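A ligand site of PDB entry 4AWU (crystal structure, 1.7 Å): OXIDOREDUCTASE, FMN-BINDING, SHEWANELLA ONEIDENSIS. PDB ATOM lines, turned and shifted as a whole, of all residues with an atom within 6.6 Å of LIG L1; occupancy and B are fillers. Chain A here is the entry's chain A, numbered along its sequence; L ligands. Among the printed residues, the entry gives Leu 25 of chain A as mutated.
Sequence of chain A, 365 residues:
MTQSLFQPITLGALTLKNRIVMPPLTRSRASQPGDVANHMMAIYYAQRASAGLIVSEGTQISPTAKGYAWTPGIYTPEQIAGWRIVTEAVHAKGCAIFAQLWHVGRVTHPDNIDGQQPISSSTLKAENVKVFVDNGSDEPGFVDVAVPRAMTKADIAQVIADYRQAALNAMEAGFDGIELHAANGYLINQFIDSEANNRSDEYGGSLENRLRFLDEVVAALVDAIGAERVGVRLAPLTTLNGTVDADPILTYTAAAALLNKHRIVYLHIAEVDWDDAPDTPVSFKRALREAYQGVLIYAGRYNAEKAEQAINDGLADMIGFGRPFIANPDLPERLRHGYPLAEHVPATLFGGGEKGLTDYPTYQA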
ATOM      1  N   PRO A  24      -4.995 -15.046  29.629  1.00  0.00           N
ATOM      2  CA  PRO A  24      -6.136 -14.232  29.210  1.00  0.00           C
ATOM      3  C   PRO A  24      -6.452 -14.460  27.740  1.00  0.00           C
ATOM      4  O   PRO A  24      -5.562 -14.374  26.901  1.00  0.00           O
ATOM      5  CB  PRO A  24      -5.657 -12.801  29.428  1.00  0.00           C
ATOM      6  CG  PRO A  24      -4.516 -12.899  30.363  1.00  0.00           C
ATOM      7  CD  PRO A  24      -3.878 -14.227  30.128  1.00  0.00           C
ATOM      8  N   LEU A  25      -7.724 -14.741  27.456  1.00  0.00           N
ATOM      9  CA  LEU A  25      -8.160 -14.940  26.088  1.00  0.00           C
ATOM     10  C   LEU A  25      -9.496 -14.241  25.855  1.00  0.00           C
ATOM     11  O   LEU A  25     -10.555 -14.760  26.205  1.00  0.00           O
ATOM     12  CB  LEU A  25      -8.292 -16.435  25.768  1.00  0.00           C
ATOM     13  CG  LEU A  25      -6.998 -17.240  25.875  1.00  0.00           C
ATOM     14  CD1 LEU A  25      -7.315 -18.706  26.098  1.00  0.00           C
ATOM     15  CD2 LEU A  25      -6.126 -17.049  24.639  1.00  0.00           C
ATOM     16  N   THR A  26      -9.424 -13.046  25.284  1.00  0.00           N
ATOM     17  CA  THR A  26     -10.586 -12.296  24.861  1.00  0.00           C
ATOM     18  C   THR A  26     -11.442 -13.142  23.926  1.00  0.00           C
ATOM     19  O   THR A  26     -10.968 -13.623  22.907  1.00  0.00           O
ATOM     20  CB  THR A  26     -10.163 -10.998  24.148  1.00  0.00           C
ATOM     21  OG1 THR A  26      -9.553 -10.125  25.103  1.00  0.00           O
ATOM     22  CG2 THR A  26     -11.342 -10.295  23.507  1.00  0.00           C
ATOM     23  N   ARG A  27     -12.707 -13.340  24.305  1.00  0.00           N
ATOM     24  CA  ARG A  27     -13.651 -14.084  23.488  1.00  0.00           C
ATOM     25  C   ARG A  27     -14.848 -13.221  23.097  1.00  0.00           C
ATOM     26  O   ARG A  27     -15.668 -13.624  22.273  1.00  0.00           O
ATOM     27  CB  ARG A  27     -14.120 -15.332  24.228  1.00  0.00           C
ATOM     28  CG  ARG A  27     -12.995 -16.198  24.791  1.00  0.00           C
ATOM     29  CD  ARG A  27     -11.986 -16.617  23.717  1.00  0.00           C
ATOM     30  NE  ARG A  27     -12.646 -17.284  22.592  1.00  0.00           N
ATOM     31  CZ  ARG A  27     -12.992 -18.564  22.576  1.00  0.00           C
ATOM     32  NH1 ARG A  27     -12.741 -19.345  23.616  1.00  0.00           N
ATOM     33  NH2 ARG A  27     -13.589 -19.074  21.516  1.00  0.00           N
ATOM     34  N   GLY A  58      -9.079 -10.085  29.174  1.00  0.00           N
ATOM     35  CA  GLY A  58      -9.050  -8.686  29.572  1.00  0.00           C
ATOM     36  C   GLY A  58     -10.442  -8.213  29.918  1.00  0.00           C
ATOM     37  O   GLY A  58     -11.397  -8.482  29.193  1.00  0.00           O
ATOM     38  N   TYR A  68     -12.826  -3.098  22.541  1.00  0.00           N
ATOM     39  CA  TYR A  68     -13.466  -3.982  21.576  1.00  0.00           C
ATOM     40  C   TYR A  68     -14.892  -4.321  21.976  1.00  0.00           C
ATOM     41  O   TYR A  68     -15.188  -4.457  23.161  1.00  0.00           O
ATOM     42  CB  TYR A  68     -12.654  -5.275  21.447  1.00  0.00           C
ATOM     43  CG  TYR A  68     -11.183  -5.048  21.211  1.00  0.00           C
ATOM     44  CD1 TYR A  68     -10.320  -4.776  22.267  1.00  0.00           C
ATOM     45  CD2 TYR A  68     -10.652  -5.108  19.933  1.00  0.00           C
ATOM     46  CE1 TYR A  68      -8.986  -4.564  22.061  1.00  0.00           C
ATOM     47  CE2 TYR A  68      -9.308  -4.901  19.713  1.00  0.00           C
ATOM     48  CZ  TYR A  68      -8.485  -4.634  20.772  1.00  0.00           C
ATOM     49  OH  TYR A  68      -7.141  -4.421  20.565  1.00  0.00           O
ATOM     50  N   GLN A 100      -7.969 -10.238  34.649  1.00  0.00           N
ATOM     51  CA  GLN A 100      -7.031  -9.361  33.956  1.00  0.00           C
ATOM     52  C   GLN A 100      -7.640  -7.981  33.777  1.00  0.00           C
ATOM     53  O   GLN A 100      -8.526  -7.783  32.937  1.00  0.00           O
ATOM     54  CB  GLN A 100      -6.600  -9.898  32.585  1.00  0.00           C
ATOM     55  CG  GLN A 100      -5.457  -9.053  32.031  1.00  0.00           C
ATOM     56  CD  GLN A 100      -5.080  -9.374  30.607  1.00  0.00           C
ATOM     57  OE1 GLN A 100      -5.919  -9.320  29.704  1.00  0.00           O
ATOM     58  NE2 GLN A 100      -3.806  -9.675  30.378  1.00  0.00           N
ATOM     59  N   TRP A 102      -8.034  -4.430  32.487  1.00  0.00           N
ATOM     60  CA  TRP A 102      -7.695  -3.930  31.174  1.00  0.00           C
ATOM     61  C   TRP A 102      -7.993  -2.453  31.011  1.00  0.00           C
ATOM     62  O   TRP A 102      -9.092  -1.990  31.337  1.00  0.00           O
ATOM     63  CB  TRP A 102      -8.528  -4.686  30.146  1.00  0.00           C
ATOM     64  CG  TRP A 102      -7.949  -4.767  28.774  1.00  0.00           C
ATOM     65  CD1 TRP A 102      -6.734  -4.303  28.354  1.00  0.00           C
ATOM     66  CD2 TRP A 102      -8.568  -5.371  27.630  1.00  0.00           C
ATOM     67  NE1 TRP A 102      -6.559  -4.591  27.019  1.00  0.00           N
ATOM     68  CE2 TRP A 102      -7.667  -5.243  26.562  1.00  0.00           C
ATOM     69  CE3 TRP A 102      -9.785  -6.011  27.426  1.00  0.00           C
ATOM     70  CZ2 TRP A 102      -7.967  -5.729  25.284  1.00  0.00           C
ATOM     71  CZ3 TRP A 102     -10.074  -6.489  26.159  1.00  0.00           C
ATOM     72  CH2 TRP A 102      -9.164  -6.352  25.102  1.00  0.00           C
ATOM     73  N   HIS A 181      -2.970  -5.822  33.041  1.00  0.00           N
ATOM     74  CA  HIS A 181      -2.621  -5.934  31.642  1.00  0.00           C
ATOM     75  C   HIS A 181      -1.736  -4.761  31.258  1.00  0.00           C
ATOM     76  O   HIS A 181      -2.220  -3.670  30.972  1.00  0.00           O
ATOM     77  CB  HIS A 181      -3.870  -5.972  30.775  1.00  0.00           C
ATOM     78  CG  HIS A 181      -3.619  -6.463  29.381  1.00  0.00           C
ATOM     79  ND1 HIS A 181      -2.346  -6.593  28.865  1.00  0.00           N
ATOM     80  CD2 HIS A 181      -4.459  -6.859  28.405  1.00  0.00           C
ATOM     81  CE1 HIS A 181      -2.423  -7.054  27.634  1.00  0.00           C
ATOM     82  NE2 HIS A 181      -3.692  -7.224  27.327  1.00  0.00           N
ATOM     83  N   ALA A 183       0.552  -5.029  28.744  1.00  0.00           N
ATOM     84  CA  ALA A 183       1.157  -5.641  27.576  1.00  0.00           C
ATOM     85  C   ALA A 183       0.408  -5.299  26.304  1.00  0.00           C
ATOM     86  O   ALA A 183      -0.567  -4.549  26.319  1.00  0.00           O
ATOM     87  CB  ALA A 183       1.221  -7.163  27.760  1.00  0.00           C
ATOM     88  N   ASN A 184       0.906  -5.846  25.194  1.00  0.00           N
ATOM     89  CA  ASN A 184       0.242  -5.759  23.900  1.00  0.00           C
ATOM     90  C   ASN A 184      -0.249  -4.367  23.537  1.00  0.00           C
ATOM     91  O   ASN A 184      -1.345  -4.210  22.986  1.00  0.00           O
ATOM     92  CB  ASN A 184      -0.893  -6.786  23.816  1.00  0.00           C
ATOM     93  CG  ASN A 184      -0.393  -8.211  23.921  1.00  0.00           C
ATOM     94  OD1 ASN A 184       0.753  -8.518  23.578  1.00  0.00           O
ATOM     95  ND2 ASN A 184      -1.251  -9.103  24.395  1.00  0.00           N
ATOM     96  N   TYR A 186      -1.308  -1.747  25.056  1.00  0.00           N
ATOM     97  CA  TYR A 186      -2.425  -1.091  25.703  1.00  0.00           C
ATOM     98  C   TYR A 186      -1.939   0.010  26.645  1.00  0.00           C
ATOM     99  O   TYR A 186      -0.755   0.362  26.624  1.00  0.00           O
ATOM    100  CB  TYR A 186      -3.333  -2.132  26.361  1.00  0.00           C
ATOM    101  CG  TYR A 186      -3.953  -3.038  25.327  1.00  0.00           C
ATOM    102  CD1 TYR A 186      -4.809  -2.529  24.356  1.00  0.00           C
ATOM    103  CD2 TYR A 186      -3.683  -4.393  25.295  1.00  0.00           C
ATOM    104  CE1 TYR A 186      -5.377  -3.345  23.402  1.00  0.00           C
ATOM    105  CE2 TYR A 186      -4.239  -5.220  24.347  1.00  0.00           C
ATOM    106  CZ  TYR A 186      -5.087  -4.686  23.403  1.00  0.00           C
ATOM    107  OH  TYR A 186      -5.653  -5.514  22.456  1.00  0.00           O
ATOM    108  N   ARG A 233       1.168  -8.515  33.659  1.00  0.00           N
ATOM    109  CA  ARG A 233       1.572  -9.104  32.391  1.00  0.00           C
ATOM    110  C   ARG A 233       2.298  -8.083  31.527  1.00  0.00           C
ATOM    111  O   ARG A 233       1.816  -6.971  31.319  1.00  0.00           O
ATOM    112  CB  ARG A 233       0.380  -9.653  31.626  1.00  0.00           C
ATOM    113  CG  ARG A 233       0.812 -10.594  30.515  1.00  0.00           C
ATOM    114  CD  ARG A 233      -0.343 -11.288  29.844  1.00  0.00           C
ATOM    115  NE  ARG A 233       0.095 -12.590  29.344  1.00  0.00           N
ATOM    116  CZ  ARG A 233      -0.459 -13.244  28.336  1.00  0.00           C
ATOM    117  NH1 ARG A 233      -1.481 -12.725  27.675  1.00  0.00           N
ATOM    118  NH2 ARG A 233       0.021 -14.426  27.988  1.00  0.00           N
ATOM    119  N   LEU A 240       2.287  -6.116  19.427  1.00  0.00           N
ATOM    120  CA  LEU A 240       0.864  -6.133  19.100  1.00  0.00           C
ATOM    121  C   LEU A 240       0.274  -4.763  19.394  1.00  0.00           C
ATOM    122  O   LEU A 240       0.462  -4.215  20.471  1.00  0.00           O
ATOM    123  CB  LEU A 240       0.144  -7.226  19.883  1.00  0.00           C
ATOM    124  CG  LEU A 240      -1.334  -7.435  19.544  1.00  0.00           C
ATOM    125  CD1 LEU A 240      -1.508  -7.673  18.058  1.00  0.00           C
ATOM    126  CD2 LEU A 240      -1.913  -8.589  20.349  1.00  0.00           C
ATOM    127  N   ASN A 241      -0.429  -4.208  18.400  1.00  0.00           N
ATOM    128  CA  ASN A 241      -1.052  -2.896  18.505  1.00  0.00           C
ATOM    129  C   ASN A 241      -0.055  -1.737  18.460  1.00  0.00           C
ATOM    130  O   ASN A 241      -0.403  -0.590  18.726  1.00  0.00           O
ATOM    131  CB  ASN A 241      -1.934  -2.807  19.742  1.00  0.00           C
ATOM    132  CG  ASN A 241      -3.056  -3.833  19.698  1.00  0.00           C
ATOM    133  OD1 ASN A 241      -3.743  -3.971  18.691  1.00  0.00           O
ATOM    134  ND2 ASN A 241      -3.212  -4.573  20.788  1.00  0.00           N
ATOM    135  N   ASP A 273       2.485 -13.310  20.017  1.00  0.00           N
ATOM    136  CA  ASP A 273       1.146 -12.834  19.716  1.00  0.00           C
ATOM    137  C   ASP A 273       0.797 -13.171  18.284  1.00  0.00           C
ATOM    138  O   ASP A 273       1.303 -12.554  17.347  1.00  0.00           O
ATOM    139  CB  ASP A 273       1.031 -11.333  19.978  1.00  0.00           C
ATOM    140  CG  ASP A 273       0.871 -11.027  21.440  1.00  0.00           C
ATOM    141  OD1 ASP A 273      -0.260 -11.191  21.951  1.00  0.00           O
ATOM    142  OD2 ASP A 273       1.873 -10.632  22.069  1.00  0.00           O
ATOM    143  N   TRP A 274      -0.051 -14.184  18.124  1.00  0.00           N
ATOM    144  CA  TRP A 274      -0.409 -14.693  16.825  1.00  0.00           C
ATOM    145  C   TRP A 274       0.879 -15.155  16.118  1.00  0.00           C
ATOM    146  O   TRP A 274       1.543 -16.077  16.596  1.00  0.00           O
ATOM    147  CB  TRP A 274      -1.171 -13.635  16.028  1.00  0.00           C
ATOM    148  CG  TRP A 274      -2.282 -12.963  16.813  1.00  0.00           C
ATOM    149  CD1 TRP A 274      -2.225 -11.746  17.432  1.00  0.00           C
ATOM    150  CD2 TRP A 274      -3.600 -13.480  17.075  1.00  0.00           C
ATOM    151  NE1 TRP A 274      -3.422 -11.467  18.052  1.00  0.00           N
ATOM    152  CE2 TRP A 274      -4.279 -12.510  17.844  1.00  0.00           C
ATOM    153  CE3 TRP A 274      -4.263 -14.660  16.731  1.00  0.00           C
ATOM    154  CZ2 TRP A 274      -5.593 -12.696  18.273  1.00  0.00           C
ATOM    155  CZ3 TRP A 274      -5.570 -14.832  17.152  1.00  0.00           C
ATOM    156  CH2 TRP A 274      -6.220 -13.855  17.910  1.00  0.00           C
ATOM    157  N   PHE A 350     -14.061 -14.739  18.517  1.00  0.00           N
ATOM    158  CA  PHE A 350     -14.682 -13.549  19.078  1.00  0.00           C
ATOM    159  C   PHE A 350     -16.146 -13.439  18.685  1.00  0.00           C
ATOM    160  O   PHE A 350     -16.500 -13.639  17.516  1.00  0.00           O
ATOM    161  CB  PHE A 350     -13.946 -12.295  18.595  1.00  0.00           C
ATOM    162  CG  PHE A 350     -12.449 -12.400  18.675  1.00  0.00           C
ATOM    163  CD1 PHE A 350     -11.812 -12.326  19.899  1.00  0.00           C
ATOM    164  CD2 PHE A 350     -11.685 -12.552  17.537  1.00  0.00           C
ATOM    165  CE1 PHE A 350     -10.439 -12.417  19.984  1.00  0.00           C
ATOM    166  CE2 PHE A 350     -10.313 -12.640  17.613  1.00  0.00           C
ATOM    167  CZ  PHE A 350      -9.694 -12.578  18.836  1.00  0.00           C
HETATM  168 CL1  LIG L   1      -7.745 -10.556  21.068  1.00  0.00          CL
HETATM  169  C1  LIG L   1      -6.541  -9.964  22.143  1.00  0.00           C
HETATM  170  C2  LIG L   1      -6.910  -9.089  23.139  1.00  0.00           C
HETATM  171  C3  LIG L   1      -5.964  -8.616  24.032  1.00  0.00           C
HETATM  172  C4  LIG L   1      -4.641  -9.011  23.909  1.00  0.00           C
HETATM  173  O1  LIG L   1      -3.724  -8.542  24.803  1.00  0.00           O
HETATM  174  C5  LIG L   1      -4.261  -9.895  22.910  1.00  0.00           C
HETATM  175  C6  LIG L   1      -5.217 -10.369  22.018  1.00  0.00           C
HETATM  176  N1  LG2 L   2      -3.539 -11.706  26.068  1.00  0.00           N
HETATM  177  C1  LG2 L   2      -3.880 -10.815  27.055  1.00  0.00           C
HETATM  178  O1  LG2 L   2      -3.000 -10.368  27.781  1.00  0.00           O
HETATM  179  N2  LG2 L   2      -5.200 -10.419  27.219  1.00  0.00           N
HETATM  180  C2  LG2 L   2      -6.169 -10.869  26.344  1.00  0.00           C
HETATM  181  O2  LG2 L   2      -7.358 -10.657  26.594  1.00  0.00           O
HETATM  182  C3  LG2 L   2      -5.825 -11.782  25.362  1.00  0.00           C
HETATM  183  N3  LG2 L   2      -6.769 -12.253  24.501  1.00  0.00           N
HETATM  184  C4  LG2 L   2      -6.428 -13.145  23.514  1.00  0.00           C
HETATM  185  C5  LG2 L   2      -7.424 -13.665  22.697  1.00  0.00           C
HETATM  186  C6  LG2 L   2      -7.124 -14.612  21.741  1.00  0.00           C
HETATM  187  C7  LG2 L   2      -8.222 -15.143  20.878  1.00  0.00           C
HETATM  188  C8  LG2 L   2      -5.793 -15.013  21.564  1.00  0.00           C
HETATM  189  C9  LG2 L   2      -5.451 -16.066  20.556  1.00  0.00           C
HETATM  190  C10 LG2 L   2      -4.804 -14.508  22.398  1.00  0.00           C
HETATM  191  C11 LG2 L   2      -5.126 -13.607  23.396  1.00  0.00           C
HETATM  192  N4  LG2 L   2      -4.150 -13.082  24.227  1.00  0.00           N
HETATM  193  C12 LG2 L   2      -4.503 -12.180  25.208  1.00  0.00           C
HETATM  194  C13 LG2 L   2      -2.744 -13.595  24.191  1.00  0.00           C
HETATM  195  C14 LG2 L   2      -2.735 -14.964  24.865  1.00  0.00           C
HETATM  196  O3  LG2 L   2      -3.033 -14.795  26.232  1.00  0.00           O
HETATM  197  C15 LG2 L   2      -1.387 -15.687  24.728  1.00  0.00           C
HETATM  198  O4  LG2 L   2      -0.406 -14.961  25.433  1.00  0.00           O
HETATM  199  C16 LG2 L   2      -1.005 -15.847  23.251  1.00  0.00           C
HETATM  200  O5  LG2 L   2      -2.089 -16.419  22.543  1.00  0.00           O
HETATM  201  C17 LG2 L   2       0.220 -16.726  23.055  1.00  0.00           C
HETATM  202  O6  LG2 L   2       0.049 -17.994  23.658  1.00  0.00           O
HETATM  203  P1  LG2 L   2      -0.315 -19.292  22.768  1.00  0.00           P
HETATM  204  O7  LG2 L   2      -1.700 -19.097  22.212  1.00  0.00           O
HETATM  205  O8  LG2 L   2       0.681 -19.438  21.641  1.00  0.00           O
HETATM  206  O9  LG2 L   2      -0.254 -20.505  23.663  1.00  0.00           O
HETATM  207 CL1  LG3 L   3     -14.096 -10.269  15.179  1.00  0.00          CL
HETATM  208  C1  LG3 L   3     -14.198  -9.486  16.717  1.00  0.00           C
HETATM  209  C2  LG3 L   3     -15.443  -9.184  17.264  1.00  0.00           C
HETATM  210  C3  LG3 L   3     -15.515  -8.587  18.503  1.00  0.00           C
HETATM  211  C4  LG3 L   3     -14.354  -8.284  19.197  1.00  0.00           C
HETATM  212  O1  LG3 L   3     -14.433  -7.712  20.450  1.00  0.00           O
HETATM  213  C5  LG3 L   3     -13.118  -8.589  18.659  1.00  0.00           C
HETATM  214  C6  LG3 L   3     -13.035  -9.195  17.418  1.00  0.00           C
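The side-chain amide nitrogen of Gln 100 is in hydrogen-bond range of an oxygen (O1) of LG2 L2, at 2.8 Å.
A ring nitrogen (NE2) of His 181 sits at hydrogen-bond distance from an oxygen (O1) of LG2 L2, at 3.3 Å.
An oxygen (O3) of LG2 L2 lies within hydrogen-bond range of the backbone carbonyl oxygen (O) of Pro 24, 2.6 Å away.
An oxygen (O4) of LG2 L2 lies within hydrogen-bond range of the guanidinium group (NH2) of Arg 233 (2.6 Å).
ND2 of Asn 184 sits at hydrogen-bond distance from O1 of LIG L1 (2.6 Å).
O2 of LG2 L2 is in hydrogen-bond range of OG1 of Thr 26 (2.7 Å).
An oxygen (O1) of LIG L1 is in hydrogen-bond range of a ring nitrogen (NE2) of His 181, 2.8 Å away.
A nitrogen (N3) of LG2 L2 is in hydrogen-bond range of the backbone NH of Thr 26.
O2 of LG2 L2 sits at hydrogen-bond distance from N of Gly 58.
A nitrogen (N2) of LG2 L2 lies close to an oxygen (O1) of LIG L1 (3.4 Å).
The side-chain hydroxyl (OH) of Tyr 186 is in hydrogen-bond range of the side-chain hydroxyl (OH) of Tyr 68 (2.6 Å).
The side-chain amide oxygen of Asn 184 lies close to the side-chain carboxylate of Asp 273, 2.8 Å away.
N of Ala 183 lies within hydrogen-bond range of ND1 of His 181, at 3.3 Å.
The backbone carbonyl oxygen (O) of Asn 184 lies within hydrogen-bond range of the side-chain amide nitrogen (ND2) of Asn 241.
The side-chain hydroxyl (OH) of Tyr 186 is in hydrogen-bond range of the side-chain amide nitrogen (ND2) of Asn 241.
Merely in contact with LIG L1: Tyr 186 (3.4 Å), Phe 350 (3.4 Å), Thr 26 (3.5 Å), Leu 240 (3.7 Å) and Trp 102 (3.7 Å).
Of the 18 residues printed, 7 come within 4 Å of LIG L1.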
